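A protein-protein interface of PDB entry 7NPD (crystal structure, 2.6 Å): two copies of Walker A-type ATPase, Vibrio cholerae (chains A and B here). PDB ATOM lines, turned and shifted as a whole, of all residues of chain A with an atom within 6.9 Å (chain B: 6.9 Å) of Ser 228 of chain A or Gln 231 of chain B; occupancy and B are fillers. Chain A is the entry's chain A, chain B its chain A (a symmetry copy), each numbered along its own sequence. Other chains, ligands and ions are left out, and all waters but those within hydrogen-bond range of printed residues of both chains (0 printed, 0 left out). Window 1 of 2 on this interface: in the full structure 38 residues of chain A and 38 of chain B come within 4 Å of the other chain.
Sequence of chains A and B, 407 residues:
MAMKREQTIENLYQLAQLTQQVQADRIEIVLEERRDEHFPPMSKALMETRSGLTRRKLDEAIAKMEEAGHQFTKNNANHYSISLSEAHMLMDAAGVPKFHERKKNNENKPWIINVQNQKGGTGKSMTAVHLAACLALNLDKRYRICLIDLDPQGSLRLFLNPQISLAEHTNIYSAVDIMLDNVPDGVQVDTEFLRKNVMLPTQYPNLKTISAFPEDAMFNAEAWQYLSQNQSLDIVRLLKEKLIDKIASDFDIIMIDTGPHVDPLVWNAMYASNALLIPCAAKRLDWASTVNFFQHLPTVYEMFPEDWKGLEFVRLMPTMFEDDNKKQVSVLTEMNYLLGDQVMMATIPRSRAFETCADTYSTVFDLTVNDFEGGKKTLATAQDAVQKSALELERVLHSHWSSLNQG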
ATOM      1  N   ALA A 223      -1.015  -9.429 -16.103  1.00  0.00           N
ATOM      2  CA  ALA A 223      -1.148 -10.330 -14.978  1.00  0.00           C
ATOM      3  C   ALA A 223      -2.583 -10.317 -14.489  1.00  0.00           C
ATOM      4  O   ALA A 223      -3.238 -11.363 -14.357  1.00  0.00           O
ATOM      5  CB  ALA A 223      -0.188  -9.902 -13.874  1.00  0.00           C
ATOM      6  N   TRP A 224      -3.076  -9.124 -14.174  1.00  0.00           N
ATOM      7  CA  TRP A 224      -4.339  -9.026 -13.459  1.00  0.00           C
ATOM      8  C   TRP A 224      -5.471  -9.407 -14.372  1.00  0.00           C
ATOM      9  O   TRP A 224      -6.583  -9.640 -13.901  1.00  0.00           O
ATOM     10  CB  TRP A 224      -4.503  -7.612 -12.894  1.00  0.00           C
ATOM     11  CG  TRP A 224      -3.508  -7.498 -11.818  1.00  0.00           C
ATOM     12  CD1 TRP A 224      -3.157  -8.489 -10.984  1.00  0.00           C
ATOM     13  CD2 TRP A 224      -2.689  -6.407 -11.516  1.00  0.00           C
ATOM     14  NE1 TRP A 224      -2.196  -8.096 -10.167  1.00  0.00           N
ATOM     15  CE2 TRP A 224      -1.871  -6.804 -10.472  1.00  0.00           C
ATOM     16  CE3 TRP A 224      -2.546  -5.141 -12.040  1.00  0.00           C
ATOM     17  CZ2 TRP A 224      -0.919  -5.965  -9.921  1.00  0.00           C
ATOM     18  CZ3 TRP A 224      -1.654  -4.303 -11.464  1.00  0.00           C
ATOM     19  CH2 TRP A 224      -0.828  -4.716 -10.427  1.00  0.00           C
ATOM     20  N   GLN A 225      -5.215  -9.468 -15.672  1.00  0.00           N
ATOM     21  CA  GLN A 225      -6.200 -10.018 -16.579  1.00  0.00           C
ATOM     22  C   GLN A 225      -5.819 -11.433 -17.030  1.00  0.00           C
ATOM     23  O   GLN A 225      -6.664 -12.151 -17.570  1.00  0.00           O
ATOM     24  CB  GLN A 225      -6.383  -9.062 -17.760  1.00  0.00           C
ATOM     25  CG  GLN A 225      -7.098  -9.648 -18.922  1.00  0.00           C
ATOM     26  CD  GLN A 225      -6.506  -9.215 -20.217  1.00  0.00           C
ATOM     27  OE1 GLN A 225      -5.382  -8.685 -20.253  1.00  0.00           O
ATOM     28  NE2 GLN A 225      -7.264  -9.405 -21.308  1.00  0.00           N
ATOM     29  N   TYR A 226      -4.604 -11.893 -16.727  1.00  0.00           N
ATOM     30  CA  TYR A 226      -4.166 -13.259 -16.974  1.00  0.00           C
ATOM     31  C   TYR A 226      -4.422 -14.126 -15.765  1.00  0.00           C
ATOM     32  O   TYR A 226      -3.891 -15.234 -15.664  1.00  0.00           O
ATOM     33  CB  TYR A 226      -2.679 -13.292 -17.338  1.00  0.00           C
ATOM     34  N   LEU A 227      -5.186 -13.605 -14.823  1.00  0.00           N
ATOM     35  CA  LEU A 227      -5.793 -14.437 -13.801  1.00  0.00           C
ATOM     36  C   LEU A 227      -7.301 -14.627 -13.978  1.00  0.00           C
ATOM     37  O   LEU A 227      -7.833 -15.649 -13.533  1.00  0.00           O
ATOM     38  CB  LEU A 227      -5.518 -13.851 -12.413  1.00  0.00           C
ATOM     39  N   SER A 228      -7.992 -13.716 -14.662  1.00  0.00           N
ATOM     40  CA  SER A 228      -9.376 -13.979 -15.042  1.00  0.00           C
ATOM     41  C   SER A 228      -9.496 -15.344 -15.681  1.00  0.00           C
ATOM     42  O   SER A 228     -10.394 -16.122 -15.343  1.00  0.00           O
ATOM     43  CB  SER A 228      -9.851 -12.925 -16.037  1.00  0.00           C
ATOM     44  OG  SER A 228      -9.002 -12.933 -17.174  1.00  0.00           O
ATOM     45  N   GLN A 229      -8.567 -15.664 -16.573  1.00  0.00           N
ATOM     46  CA  GLN A 229      -8.500 -16.966 -17.203  1.00  0.00           C
ATOM     47  C   GLN A 229      -7.798 -17.982 -16.319  1.00  0.00           C
ATOM     48  O   GLN A 229      -7.542 -19.102 -16.774  1.00  0.00           O
ATOM     49  CB  GLN A 229      -7.782 -16.861 -18.553  1.00  0.00           C
ATOM     50  N   ASN A 230      -7.453 -17.611 -15.080  1.00  0.00           N
ATOM     51  CA  ASN A 230      -6.855 -18.592 -14.183  1.00  0.00           C
ATOM     52  C   ASN A 230      -6.653 -18.131 -12.744  1.00  0.00           C
ATOM     53  O   ASN A 230      -5.976 -17.129 -12.520  1.00  0.00           O
ATOM     54  CB  ASN A 230      -5.518 -19.016 -14.757  1.00  0.00           C
ATOM     55  N   GLN A 231      -7.162 -18.864 -11.757  1.00  0.00           N
ATOM     56  CA  GLN A 231      -6.711 -18.661 -10.379  1.00  0.00           C
ATOM     57  C   GLN A 231      -5.491 -19.534 -10.179  1.00  0.00           C
ATOM     58  O   GLN A 231      -5.423 -20.412  -9.316  1.00  0.00           O
ATOM     59  CB  GLN A 231      -7.798 -19.012  -9.371  1.00  0.00           C
ATOM     60  N   TYR B 226      -8.329 -11.641  -3.810  1.00  0.00           N
ATOM     61  CA  TYR B 226      -9.783 -11.687  -3.829  1.00  0.00           C
ATOM     62  C   TYR B 226     -10.290 -11.881  -5.237  1.00  0.00           C
ATOM     63  O   TYR B 226     -11.476 -11.682  -5.510  1.00  0.00           O
ATOM     64  CB  TYR B 226     -10.372 -10.407  -3.230  1.00  0.00           C
ATOM     65  N   LEU B 227      -9.389 -12.211  -6.143  1.00  0.00           N
ATOM     66  CA  LEU B 227      -9.781 -12.766  -7.427  1.00  0.00           C
ATOM     67  C   LEU B 227      -9.486 -14.260  -7.567  1.00  0.00           C
ATOM     68  O   LEU B 227     -10.177 -14.939  -8.331  1.00  0.00           O
ATOM     69  CB  LEU B 227      -9.087 -12.005  -8.561  1.00  0.00           C
ATOM     70  N   SER B 228      -8.530 -14.805  -6.813  1.00  0.00           N
ATOM     71  CA  SER B 228      -8.380 -16.255  -6.755  1.00  0.00           C
ATOM     72  C   SER B 228      -9.717 -16.913  -6.497  1.00  0.00           C
ATOM     73  O   SER B 228     -10.080 -17.887  -7.164  1.00  0.00           O
ATOM     74  CB  SER B 228      -7.418 -16.633  -5.633  1.00  0.00           C
ATOM     75  OG  SER B 228      -7.906 -16.123  -4.402  1.00  0.00           O
ATOM     76  N   GLN B 229     -10.477 -16.359  -5.561  1.00  0.00           N
ATOM     77  CA  GLN B 229     -11.816 -16.824  -5.264  1.00  0.00           C
ATOM     78  C   GLN B 229     -12.838 -16.252  -6.231  1.00  0.00           C
ATOM     79  O   GLN B 229     -14.040 -16.446  -6.023  1.00  0.00           O
ATOM     80  CB  GLN B 229     -12.193 -16.455  -3.824  1.00  0.00           C
ATOM     81  N   ASN B 230     -12.392 -15.524  -7.264  1.00  0.00           N
ATOM     82  CA  ASN B 230     -13.345 -15.035  -8.253  1.00  0.00           C
ATOM     83  C   ASN B 230     -12.733 -14.367  -9.479  1.00  0.00           C
ATOM     84  O   ASN B 230     -11.991 -13.398  -9.332  1.00  0.00           O
ATOM     85  CB  ASN B 230     -14.282 -14.057  -7.574  1.00  0.00           C
ATOM     86  N   GLN B 231     -13.071 -14.810 -10.688  1.00  0.00           N
ATOM     87  CA  GLN B 231     -12.794 -14.000 -11.875  1.00  0.00           C
ATOM     88  C   GLN B 231     -13.973 -13.072 -12.065  1.00  0.00           C
ATOM     89  O   GLN B 231     -14.659 -13.053 -13.089  1.00  0.00           O
ATOM     90  CB  GLN B 231     -12.581 -14.865 -13.112  1.00  0.00           C
ATOM     91  N   SER B 232     -14.236 -12.347 -10.978  1.00  0.00           N
ATOM     92  CA  SER B 232     -15.554 -11.810 -10.653  1.00  0.00           C
ATOM     93  C   SER B 232     -15.826 -10.443 -11.253  1.00  0.00           C
ATOM     94  O   SER B 232     -16.623 -10.317 -12.188  1.00  0.00           O
ATOM     95  CB  SER B 232     -15.641 -11.688  -9.143  1.00  0.00           C
ATOM     96  OG  SER B 232     -16.855 -11.177  -8.637  1.00  0.00           O
ATOM     97  N   LEU B 233     -15.150  -9.431 -10.712  1.00  0.00           N
ATOM     98  CA  LEU B 233     -15.172  -8.028 -11.146  1.00  0.00           C
ATOM     99  C   LEU B 233     -16.283  -7.217 -10.470  1.00  0.00           C
ATOM    100  O   LEU B 233     -16.993  -6.420 -11.096  1.00  0.00           O
ATOM    101  CB  LEU B 233     -15.226  -7.889 -12.658  1.00  0.00           C
ATOM    102  CG  LEU B 233     -13.875  -8.104 -13.333  1.00  0.00           C
ATOM    103  CD1 LEU B 233     -13.366  -6.777 -12.964  1.00  0.00           C
ATOM    104  CD2 LEU B 233     -12.914  -9.188 -12.876  1.00  0.00           C
ATOM    105  N   ASP B 234     -16.405  -7.424  -9.159  1.00  0.00           N
ATOM    106  CA  ASP B 234     -17.171  -6.606  -8.229  1.00  0.00           C
ATOM    107  C   ASP B 234     -16.255  -5.828  -7.292  1.00  0.00           C
ATOM    108  O   ASP B 234     -16.731  -5.136  -6.388  1.00  0.00           O
ATOM    109  CB  ASP B 234     -18.068  -7.517  -7.407  1.00  0.00           C
ATOM    110  CG  ASP B 234     -19.085  -8.233  -8.245  1.00  0.00           C
ATOM    111  OD1 ASP B 234     -19.196  -9.465  -8.088  1.00  0.00           O
ATOM    112  OD2 ASP B 234     -19.796  -7.575  -9.029  1.00  0.00           O
ATOM    113  N   MET B 303     -13.686  -4.097 -18.468  1.00  0.00           N
ATOM    114  CA  MET B 303     -13.732  -5.148 -17.506  1.00  0.00           C
ATOM    115  C   MET B 303     -14.798  -4.928 -16.410  1.00  0.00           C
ATOM    116  O   MET B 303     -15.313  -5.923 -15.869  1.00  0.00           O
ATOM    117  CB  MET B 303     -12.279  -5.226 -17.017  1.00  0.00           C
ATOM    118  CG  MET B 303     -11.929  -6.269 -15.952  1.00  0.00           C
ATOM    119  SD  MET B 303     -10.290  -6.386 -15.211  1.00  0.00           S
ATOM    120  CE  MET B 303      -9.263  -6.653 -16.618  1.00  0.00           C
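Trp 224 of chain A touches none of the printed residues of chain B.
Ser 228 of chain A touches just one residue of chain B: Gln 231.
Of the printed residues of chain B, Gln 231 of chain A touches Ser 228.
Tyr 226 of chain B touches none of the printed residues of chain A.
Of the printed residues of chain A, Ser 228 of chain B touches Gln 231 (3.4 Å).
The nearest residue of chain B that does not touch Ser 228 of chain A is Leu 233 of chain B (5.8 Å).
The nearest residue of chain A that does not touch Gln 231 of chain B is Leu 227 of chain A (4.8 Å).
Of the 9 printed residues of chain A, 3 touch a printed residue of chain B.
Hydrophobic or aromatic side chains of chain B that line the printed part of chain A: Met 303.
Along chain B the printed residues that touch a printed residue of chain A span positions 228 to 303.
O of Gln 225 of chain A sits at hydrogen-bond distance from OG of Ser 228 of chain A.
Ser 228 of chain A touches Gln 231 of chain B, and with the chains exchanged Gln 231 of chain A touches Ser 228 of chain B.
Positions printed for both chains: 226, 227, 228, 229, 230 and 231.
Of the 3 pairs that touch across the chains among the printed residues, 2 have their exchanged pair printed and touching as well.
Among the printed residues, pairs that only touch across the chains: Gln 225 of chain A with Met 303 of chain B, Ser 228 of chain A with Gln 231 of chain B and Gln 231 of chain A with Ser 228 of chain B.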
